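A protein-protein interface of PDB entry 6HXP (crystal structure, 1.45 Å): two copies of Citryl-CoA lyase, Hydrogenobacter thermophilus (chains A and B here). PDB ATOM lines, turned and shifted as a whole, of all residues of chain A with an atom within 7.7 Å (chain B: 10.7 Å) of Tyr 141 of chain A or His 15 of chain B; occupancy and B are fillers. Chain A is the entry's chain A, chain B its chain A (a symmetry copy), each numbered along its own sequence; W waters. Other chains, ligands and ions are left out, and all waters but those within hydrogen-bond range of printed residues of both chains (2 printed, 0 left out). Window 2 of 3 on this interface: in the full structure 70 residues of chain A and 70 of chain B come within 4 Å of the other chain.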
ATOM      1  N   HIS A  64      14.781   3.584 -25.996  1.00  0.00           N
ATOM      2  CA  HIS A  64      14.942   2.130 -25.888  1.00  0.00           C
ATOM      3  C   HIS A  64      15.196   1.726 -24.455  1.00  0.00           C
ATOM      4  O   HIS A  64      15.814   0.698 -24.199  1.00  0.00           O
ATOM      5  CB  HIS A  64      16.052   1.624 -26.820  1.00  0.00           C
ATOM      6  CG  HIS A  64      15.847   0.187 -27.217  1.00  0.00           C
ATOM      7  ND1 HIS A  64      16.529  -0.854 -26.587  1.00  0.00           N
ATOM      8  CD2 HIS A  64      14.952  -0.345 -28.065  1.00  0.00           C
ATOM      9  CE1 HIS A  64      16.079  -1.971 -27.145  1.00  0.00           C
ATOM     10  NE2 HIS A  64      15.141  -1.714 -28.052  1.00  0.00           N
ATOM     11  N   GLY A 138      20.085  -9.052 -39.235  1.00  0.00           N
ATOM     12  CA  GLY A 138      20.225  -9.882 -38.056  1.00  0.00           C
ATOM     13  C   GLY A 138      19.727  -9.267 -36.767  1.00  0.00           C
ATOM     14  O   GLY A 138      19.767  -8.057 -36.581  1.00  0.00           O
ATOM     15  N   HIS A 139      19.304 -10.131 -35.828  1.00  0.00           N
ATOM     16  CA  HIS A 139      18.820  -9.702 -34.516  1.00  0.00           C
ATOM     17  C   HIS A 139      19.008 -10.846 -33.533  1.00  0.00           C
ATOM     18  O   HIS A 139      18.867 -11.995 -33.926  1.00  0.00           O
ATOM     19  CB  HIS A 139      17.335  -9.325 -34.593  1.00  0.00           C
ATOM     20  CG  HIS A 139      16.838  -8.564 -33.400  1.00  0.00           C
ATOM     21  ND1 HIS A 139      16.446  -9.214 -32.232  1.00  0.00           N
ATOM     22  CD2 HIS A 139      16.678  -7.233 -33.232  1.00  0.00           C
ATOM     23  CE1 HIS A 139      16.045  -8.256 -31.405  1.00  0.00           C
ATOM     24  NE2 HIS A 139      16.145  -7.045 -31.974  1.00  0.00           N
ATOM     25  N   ARG A 140      19.334 -10.537 -32.277  1.00  0.00           N
ATOM     26  CA  ARG A 140      19.550 -11.576 -31.252  1.00  0.00           C
ATOM     27  C   ARG A 140      18.302 -12.423 -30.974  1.00  0.00           C
ATOM     28  O   ARG A 140      18.425 -13.610 -30.660  1.00  0.00           O
ATOM     29  CB  ARG A 140      20.045 -10.963 -29.922  1.00  0.00           C
ATOM     30  CG  ARG A 140      21.522 -10.564 -29.872  1.00  0.00           C
ATOM     31  CD  ARG A 140      22.490 -11.746 -29.849  1.00  0.00           C
ATOM     32  NE  ARG A 140      22.306 -12.609 -28.675  1.00  0.00           N
ATOM     33  CZ  ARG A 140      22.250 -13.940 -28.711  1.00  0.00           C
ATOM     34  NH1 ARG A 140      22.368 -14.587 -29.865  1.00  0.00           N
ATOM     35  NH2 ARG A 140      22.078 -14.633 -27.593  1.00  0.00           N
ATOM     36  N   TYR A 141      17.118 -11.812 -31.026  1.00  0.00           N
ATOM     37  CA  TYR A 141      15.840 -12.476 -30.745  1.00  0.00           C
ATOM     38  C   TYR A 141      14.983 -12.722 -31.984  1.00  0.00           C
ATOM     39  O   TYR A 141      14.435 -13.802 -32.136  1.00  0.00           O
ATOM     40  CB  TYR A 141      15.053 -11.631 -29.724  1.00  0.00           C
ATOM     41  CG  TYR A 141      13.682 -12.178 -29.392  1.00  0.00           C
ATOM     42  CD1 TYR A 141      13.537 -13.356 -28.667  1.00  0.00           C
ATOM     43  CD2 TYR A 141      12.527 -11.527 -29.814  1.00  0.00           C
ATOM     44  CE1 TYR A 141      12.277 -13.856 -28.341  1.00  0.00           C
ATOM     45  CE2 TYR A 141      11.261 -12.022 -29.503  1.00  0.00           C
ATOM     46  CZ  TYR A 141      11.141 -13.186 -28.764  1.00  0.00           C
ATOM     47  OH  TYR A 141       9.893 -13.677 -28.468  1.00  0.00           O
ATOM     48  N   TYR A 142      14.785 -11.702 -32.826  1.00  0.00           N
ATOM     49  CA  TYR A 142      13.910 -11.839 -33.989  1.00  0.00           C
ATOM     50  C   TYR A 142      14.570 -12.621 -35.107  1.00  0.00           C
ATOM     51  O   TYR A 142      15.539 -12.159 -35.695  1.00  0.00           O
ATOM     52  CB  TYR A 142      13.489 -10.459 -34.503  1.00  0.00           C
ATOM     53  CG  TYR A 142      12.645  -9.703 -33.505  1.00  0.00           C
ATOM     54  CD1 TYR A 142      11.449 -10.230 -33.032  1.00  0.00           C
ATOM     55  CD2 TYR A 142      13.028  -8.448 -33.050  1.00  0.00           C
ATOM     56  CE1 TYR A 142      10.668  -9.541 -32.110  1.00  0.00           C
ATOM     57  CE2 TYR A 142      12.289  -7.780 -32.070  1.00  0.00           C
ATOM     58  CZ  TYR A 142      11.083  -8.301 -31.650  1.00  0.00           C
ATOM     59  OH  TYR A 142      10.316  -7.607 -30.748  1.00  0.00           O
ATOM     60  N   LYS A 143      14.050 -13.818 -35.380  1.00  0.00           N
ATOM     61  CA  LYS A 143      14.575 -14.702 -36.423  1.00  0.00           C
ATOM     62  C   LYS A 143      13.608 -14.870 -37.585  1.00  0.00           C
ATOM     63  O   LYS A 143      13.956 -15.585 -38.516  1.00  0.00           O
ATOM     64  CB  LYS A 143      14.878 -16.082 -35.839  1.00  0.00           C
ATOM     65  CG  LYS A 143      15.719 -16.078 -34.572  1.00  0.00           C
ATOM     66  CD  LYS A 143      17.068 -15.402 -34.744  1.00  0.00           C
ATOM     67  CE  LYS A 143      17.899 -15.524 -33.499  1.00  0.00           C
ATOM     68  NZ  LYS A 143      19.139 -14.723 -33.593  1.00  0.00           N
ATOM     69  N   ASP A 144      12.374 -14.352 -37.483  1.00  0.00           N
ATOM     70  CA  ASP A 144      11.354 -14.421 -38.550  1.00  0.00           C
ATOM     71  C   ASP A 144      11.281 -13.060 -39.211  1.00  0.00           C
ATOM     72  O   ASP A 144      11.446 -12.921 -40.425  1.00  0.00           O
ATOM     73  CB  ASP A 144       9.981 -14.824 -37.947  1.00  0.00           C
ATOM     74  CG  ASP A 144       8.822 -14.972 -38.922  1.00  0.00           C
ATOM     75  OD1 ASP A 144       9.055 -14.874 -40.146  1.00  0.00           O
ATOM     76  OD2 ASP A 144       7.670 -15.165 -38.453  1.00  0.00           O
ATOM     77  N   PHE A 145      11.007 -12.044 -38.404  1.00  0.00           N
ATOM     78  CA  PHE A 145      10.970 -10.663 -38.881  1.00  0.00           C
ATOM     79  C   PHE A 145      11.124  -9.746 -37.705  1.00  0.00           C
ATOM     80  O   PHE A 145      10.796 -10.129 -36.577  1.00  0.00           O
ATOM     81  CB  PHE A 145       9.662 -10.317 -39.637  1.00  0.00           C
ATOM     82  CG  PHE A 145       8.395 -10.356 -38.805  1.00  0.00           C
ATOM     83  CD1 PHE A 145       7.713 -11.544 -38.605  1.00  0.00           C
ATOM     84  CD2 PHE A 145       7.902  -9.206 -38.207  1.00  0.00           C
ATOM     85  CE1 PHE A 145       6.555 -11.581 -37.824  1.00  0.00           C
ATOM     86  CE2 PHE A 145       6.733  -9.236 -37.459  1.00  0.00           C
ATOM     87  CZ  PHE A 145       6.062 -10.419 -37.276  1.00  0.00           C
ATOM     88  N   PRO A 147       9.638  -6.750 -35.948  1.00  0.00           N
ATOM     89  CA  PRO A 147       8.338  -6.057 -36.031  1.00  0.00           C
ATOM     90  C   PRO A 147       8.460  -4.558 -36.290  1.00  0.00           C
ATOM     91  O   PRO A 147       7.572  -3.951 -36.861  1.00  0.00           O
ATOM     92  CB  PRO A 147       7.661  -6.345 -34.701  1.00  0.00           C
ATOM     93  CG  PRO A 147       8.607  -7.030 -33.879  1.00  0.00           C
ATOM     94  CD  PRO A 147       9.816  -7.417 -34.645  1.00  0.00           C
ATOM     95  N   ARG A 148       9.587  -3.975 -35.917  1.00  0.00           N
ATOM     96  CA  ARG A 148       9.797  -2.551 -36.122  1.00  0.00           C
ATOM     97  C   ARG A 148      10.031  -2.255 -37.605  1.00  0.00           C
ATOM     98  O   ARG A 148       9.547  -1.252 -38.141  1.00  0.00           O
ATOM     99  CB  ARG A 148      10.967  -2.075 -35.278  1.00  0.00           C
ATOM    100  CG  ARG A 148      10.777  -2.344 -33.781  1.00  0.00           C
ATOM    101  CD  ARG A 148      12.062  -2.285 -32.994  1.00  0.00           C
ATOM    102  NE  ARG A 148      13.029  -3.282 -33.453  1.00  0.00           N
ATOM    103  CZ  ARG A 148      14.288  -3.321 -33.028  1.00  0.00           C
ATOM    104  NH1 ARG A 148      14.706  -2.472 -32.094  1.00  0.00           N
ATOM    105  NH2 ARG A 148      15.141  -4.199 -33.538  1.00  0.00           N
ATOM    106  N   VAL A 185      16.940 -11.396 -40.304  1.00  0.00           N
ATOM    107  CA  VAL A 185      15.964 -10.325 -40.548  1.00  0.00           C
ATOM    108  C   VAL A 185      16.594  -9.032 -41.000  1.00  0.00           C
ATOM    109  O   VAL A 185      17.699  -8.690 -40.569  1.00  0.00           O
ATOM    110  CB  VAL A 185      15.074 -10.094 -39.295  1.00  0.00           C
ATOM    111  CG1 VAL A 185      14.422 -11.396 -38.815  1.00  0.00           C
ATOM    112  CG2 VAL A 185      15.833  -9.414 -38.175  1.00  0.00           C
ATOM    113  N   THR B  10      10.216   3.897 -20.012  1.00  0.00           N
ATOM    114  CA  THR B  10      10.093   2.844 -21.019  1.00  0.00           C
ATOM    115  C   THR B  10      10.304   1.478 -20.386  1.00  0.00           C
ATOM    116  O   THR B  10      11.081   1.352 -19.452  1.00  0.00           O
ATOM    117  CB  THR B  10      11.187   3.089 -22.096  1.00  0.00           C
ATOM    118  OG1 THR B  10      10.973   4.338 -22.751  1.00  0.00           O
ATOM    119  CG2 THR B  10      11.309   1.981 -23.145  1.00  0.00           C
ATOM    120  N   GLN B  11       9.612   0.474 -20.927  1.00  0.00           N
ATOM    121  CA  GLN B  11       9.886  -0.902 -20.573  1.00  0.00           C
ATOM    122  C   GLN B  11       9.679  -1.771 -21.760  1.00  0.00           C
ATOM    123  O   GLN B  11       9.038  -1.349 -22.726  1.00  0.00           O
ATOM    124  CB  GLN B  11       9.140  -1.415 -19.354  1.00  0.00           C
ATOM    125  CG  GLN B  11       7.692  -1.574 -19.506  1.00  0.00           C
ATOM    126  CD  GLN B  11       7.073  -2.431 -18.372  1.00  0.00           C
ATOM    127  OE1 GLN B  11       7.706  -3.216 -17.608  1.00  0.00           O
ATOM    128  NE2 GLN B  11       5.852  -2.185 -18.166  1.00  0.00           N
ATOM    129  N   HIS B  12      10.228  -2.973 -21.708  1.00  0.00           N
ATOM    130  CA  HIS B  12      10.057  -3.952 -22.768  1.00  0.00           C
ATOM    131  C   HIS B  12       9.199  -5.095 -22.254  1.00  0.00           C
ATOM    132  O   HIS B  12       9.420  -5.572 -21.147  1.00  0.00           O
ATOM    133  CB  HIS B  12      11.409  -4.440 -23.283  1.00  0.00           C
ATOM    134  CG  HIS B  12      12.127  -3.369 -24.034  1.00  0.00           C
ATOM    135  ND1 HIS B  12      12.868  -2.415 -23.371  1.00  0.00           N
ATOM    136  CD2 HIS B  12      12.078  -3.058 -25.351  1.00  0.00           C
ATOM    137  CE1 HIS B  12      13.262  -1.552 -24.307  1.00  0.00           C
ATOM    138  NE2 HIS B  12      12.816  -1.906 -25.517  1.00  0.00           N
ATOM    139  N   ILE B  13       8.191  -5.466 -23.026  1.00  0.00           N
ATOM    140  CA  ILE B  13       7.315  -6.609 -22.712  1.00  0.00           C
ATOM    141  C   ILE B  13       7.409  -7.499 -23.945  1.00  0.00           C
ATOM    142  O   ILE B  13       7.015  -7.062 -25.021  1.00  0.00           O
ATOM    143  CB  ILE B  13       5.903  -6.101 -22.426  1.00  0.00           C
ATOM    144  CG1 ILE B  13       5.868  -5.288 -21.113  1.00  0.00           C
ATOM    145  CG2 ILE B  13       4.930  -7.289 -22.284  1.00  0.00           C
ATOM    146  CD1 ILE B  13       4.827  -4.302 -21.165  1.00  0.00           C
ATOM    147  N   GLY B  14       8.019  -8.675 -23.799  1.00  0.00           N
ATOM    148  CA  GLY B  14       8.186  -9.633 -24.897  1.00  0.00           C
ATOM    149  C   GLY B  14       9.026  -9.094 -26.046  1.00  0.00           C
ATOM    150  O   GLY B  14       8.670  -9.279 -27.219  1.00  0.00           O
ATOM    151  N   HIS B  15      10.126  -8.396 -25.698  1.00  0.00           N
ATOM    152  CA  HIS B  15      11.064  -7.688 -26.584  1.00  0.00           C
ATOM    153  C   HIS B  15      10.453  -6.422 -27.251  1.00  0.00           C
ATOM    154  O   HIS B  15      11.195  -5.665 -27.861  1.00  0.00           O
ATOM    155  CB  HIS B  15      11.719  -8.602 -27.640  1.00  0.00           C
ATOM    156  CG  HIS B  15      12.696  -9.566 -27.042  1.00  0.00           C
ATOM    157  ND1 HIS B  15      12.290 -10.800 -26.561  1.00  0.00           N
ATOM    158  CD2 HIS B  15      14.025  -9.424 -26.825  1.00  0.00           C
ATOM    159  CE1 HIS B  15      13.379 -11.371 -26.065  1.00  0.00           C
ATOM    160  NE2 HIS B  15      14.453 -10.584 -26.213  1.00  0.00           N
ATOM    161  N   GLU B  16       9.151  -6.146 -27.073  1.00  0.00           N
ATOM    162  CA  GLU B  16       8.532  -4.952 -27.659  1.00  0.00           C
ATOM    163  C   GLU B  16       8.679  -3.750 -26.723  1.00  0.00           C
ATOM    164  O   GLU B  16       8.456  -3.894 -25.526  1.00  0.00           O
ATOM    165  CB  GLU B  16       7.051  -5.179 -27.966  1.00  0.00           C
ATOM    166  CG  GLU B  16       6.844  -6.164 -29.094  1.00  0.00           C
ATOM    167  CD  GLU B  16       5.443  -6.179 -29.664  1.00  0.00           C
ATOM    168  OE1 GLU B  16       4.488  -5.872 -28.912  1.00  0.00           O
ATOM    169  OE2 GLU B  16       5.300  -6.523 -30.860  1.00  0.00           O
ATOM    170  N   THR B  17       8.964  -2.579 -27.281  1.00  0.00           N
ATOM    171  CA  THR B  17       9.159  -1.377 -26.529  1.00  0.00           C
ATOM    172  C   THR B  17       7.813  -0.726 -26.233  1.00  0.00           C
ATOM    173  O   THR B  17       6.984  -0.562 -27.118  1.00  0.00           O
ATOM    174  CB  THR B  17      10.032  -0.401 -27.320  1.00  0.00           C
ATOM    175  OG1 THR B  17      11.271  -1.037 -27.721  1.00  0.00           O
ATOM    176  CG2 THR B  17      10.328   0.865 -26.559  1.00  0.00           C
ATOM    177  N   TYR B  18       7.626  -0.335 -24.969  1.00  0.00           N
ATOM    178  CA  TYR B  18       6.478   0.438 -24.518  1.00  0.00           C
ATOM    179  C   TYR B  18       6.993   1.754 -23.985  1.00  0.00           C
ATOM    180  O   TYR B  18       7.901   1.762 -23.130  1.00  0.00           O
ATOM    181  CB  TYR B  18       5.711  -0.305 -23.419  1.00  0.00           C
ATOM    182  CG  TYR B  18       4.843  -1.398 -23.992  1.00  0.00           C
ATOM    183  CD1 TYR B  18       5.408  -2.524 -24.580  1.00  0.00           C
ATOM    184  CD2 TYR B  18       3.466  -1.243 -24.082  1.00  0.00           C
ATOM    185  CE1 TYR B  18       4.610  -3.510 -25.167  1.00  0.00           C
ATOM    186  CE2 TYR B  18       2.673  -2.213 -24.672  1.00  0.00           C
ATOM    187  CZ  TYR B  18       3.249  -3.315 -25.248  1.00  0.00           C
ATOM    188  OH  TYR B  18       2.396  -4.214 -25.859  1.00  0.00           O
ATOM    189  N   ILE B  19       6.485   2.856 -24.508  1.00  0.00           N
ATOM    190  CA  ILE B  19       6.845   4.211 -24.121  1.00  0.00           C
ATOM    191  C   ILE B  19       5.714   4.750 -23.247  1.00  0.00           C
ATOM    192  O   ILE B  19       4.620   4.956 -23.778  1.00  0.00           O
ATOM    193  CB  ILE B  19       7.013   5.127 -25.362  1.00  0.00           C
ATOM    194  CG1 ILE B  19       8.049   4.580 -26.353  1.00  0.00           C
ATOM    195  CG2 ILE B  19       7.359   6.565 -24.927  1.00  0.00           C
ATOM    196  CD1 ILE B  19       9.422   4.518 -25.914  1.00  0.00           C
ATOM    197  N   ARG B  23       2.419   0.952 -26.630  1.00  0.00           N
ATOM    198  CA  ARG B  23       3.232   0.138 -27.539  1.00  0.00           C
ATOM    199  C   ARG B  23       3.858   1.059 -28.588  1.00  0.00           C
ATOM    200  O   ARG B  23       3.140   1.711 -29.362  1.00  0.00           O
ATOM    201  CB  ARG B  23       2.346  -0.895 -28.185  1.00  0.00           C
ATOM    202  CG  ARG B  23       3.065  -1.866 -29.071  1.00  0.00           C
ATOM    203  CD  ARG B  23       2.041  -2.862 -29.628  1.00  0.00           C
ATOM    204  NE  ARG B  23       2.694  -3.864 -30.462  1.00  0.00           N
ATOM    205  CZ  ARG B  23       2.488  -4.020 -31.766  1.00  0.00           C
ATOM    206  NH1 ARG B  23       1.641  -3.229 -32.412  1.00  0.00           N
ATOM    207  NH2 ARG B  23       3.139  -4.961 -32.437  1.00  0.00           N
ATOM    208  N   LEU B  24       5.196   1.094 -28.635  1.00  0.00           N
ATOM    209  CA  LEU B  24       5.879   1.980 -29.591  1.00  0.00           C
ATOM    210  C   LEU B  24       5.436   1.702 -31.024  1.00  0.00           C
ATOM    211  O   LEU B  24       5.194   2.660 -31.760  1.00  0.00           O
ATOM    212  CB  LEU B  24       7.382   1.862 -29.431  1.00  0.00           C
ATOM    213  CG  LEU B  24       8.200   2.816 -30.372  1.00  0.00           C
ATOM    214  CD1 LEU B  24       7.728   4.247 -30.285  1.00  0.00           C
ATOM    215  CD2 LEU B  24       9.663   2.750 -30.020  1.00  0.00           C
ATOM    216  N   LEU B  25       5.230   0.443 -31.393  1.00  0.00           N
ATOM    217  CA  LEU B  25       4.808   0.129 -32.747  1.00  0.00           C
ATOM    218  C   LEU B  25       3.439   0.675 -33.085  1.00  0.00           C
ATOM    219  O   LEU B  25       3.171   0.908 -34.271  1.00  0.00           O
ATOM    220  CB  LEU B  25       4.955  -1.352 -33.032  1.00  0.00           C
ATOM    221  CG  LEU B  25       6.495  -1.700 -33.152  1.00  0.00           C
ATOM    222  CD1 LEU B  25       6.690  -2.965 -33.702  1.00  0.00           C
ATOM    223  CD2 LEU B  25       7.292  -0.677 -34.015  1.00  0.00           C
HETATM  224  O   HOH W   1       8.143  -8.988 -29.991  1.00  0.00           O
HETATM  225  O   HOH W   2      12.584  -0.528 -30.164  1.00  0.00           O
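Among the printed residues, merely in contact across the chains: Tyr 141 of chain A with His 15 of chain B (3.3 Å), Pro 147 of chain A with Leu 25 of chain B (3.4 Å), Tyr 142 of chain A with His 15 of chain B (3.6 Å), His 64 of chain A with Thr 17 of chain B (3.8 Å) and Arg 148 of chain A with Leu 25 of chain B (3.8 Å).
No position is printed for both chains.
Of the 6 pairs that touch across the chains among the printed residues, none has its exchanged pair printed and touching as well.
ND1 of His 139 of chain A is in hydrogen-bond range of N of Tyr 142 of chain A.
NE2 of His 139 of chain A sits at hydrogen-bond distance from NH2 of Arg 148 of chain A (3.4 Å).
A ring nitrogen (NE2) of His 12 of chain B lies within hydrogen-bond range of the side-chain hydroxyl of Thr 17 of chain B, at 2.8 Å.
The backbone NH (N) of Tyr 141 of chain A is in hydrogen-bond range of a ring nitrogen (ND1) of His 139 of chain A, at 2.9 Å.
O of Thr 17 of chain B sits at hydrogen-bond distance from N of Leu 24 of chain B (2.9 Å).
Of chain B, only His 15 comes within 4 Å of Tyr 141 of chain A.
Of chain A, only Tyr 141 (3.3 Å) and Tyr 142 (3.6 Å) come within 4 Å of His 15 of chain B.
No residue of chain B comes within 4 Å of His 139 of chain A.
Of chain B, only His 15 comes within 4 Å of Tyr 142 of chain A.
No residue of chain B comes within 4 Å of Lys 143 of chain A.
No residue of chain A comes within 4 Å of Gly 14 of chain B.
Of the printed residues of chain B, Arg 148 of chain A touches Leu 25.
Of the printed residues of chain B, His 64 of chain A touches His 12 (3.4 Å) and Thr 17 (3.8 Å).
The nearest residue of chain B that does not touch Tyr 141 of chain A is Gly 14 of chain B (4.4 Å).
The nearest residue of chain A that does not touch His 15 of chain B is His 139 of chain A (5.1 Å).
The nearest printed residue of chain B that does not touch His 64 of chain A is Thr 10 of chain B (4.1 Å).
A ring nitrogen (NE2) of His 12 of chain B lies within hydrogen-bond range of a ring nitrogen (NE2) of His 64 of chain A (3.4 Å).
Of the 13 printed residues of chain B, 4 touch a printed residue of chain A.
Hydrophobic or aromatic side chains of chain B that line the printed part of chain A: His 12, His 15 and Leu 25.
Printed residues of chain A that touch a printed residue of chain B: His 64, Tyr 141, Tyr 142, Pro 147 and Arg 148.
Along chain A the printed residues that touch a printed residue of chain B span positions 64 to 148.
Among the printed residues, 6 pairs touch across the chains.
Water W1 lies within hydrogen-bond range of the side-chain hydroxyl of Tyr 142 of chain A and the backbone carbonyl oxygen of Gly 14 of chain B.
Water W2 lies within hydrogen-bond range of OG1 of Thr 17 of chain B and NH1 of Arg 148 of chain A.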
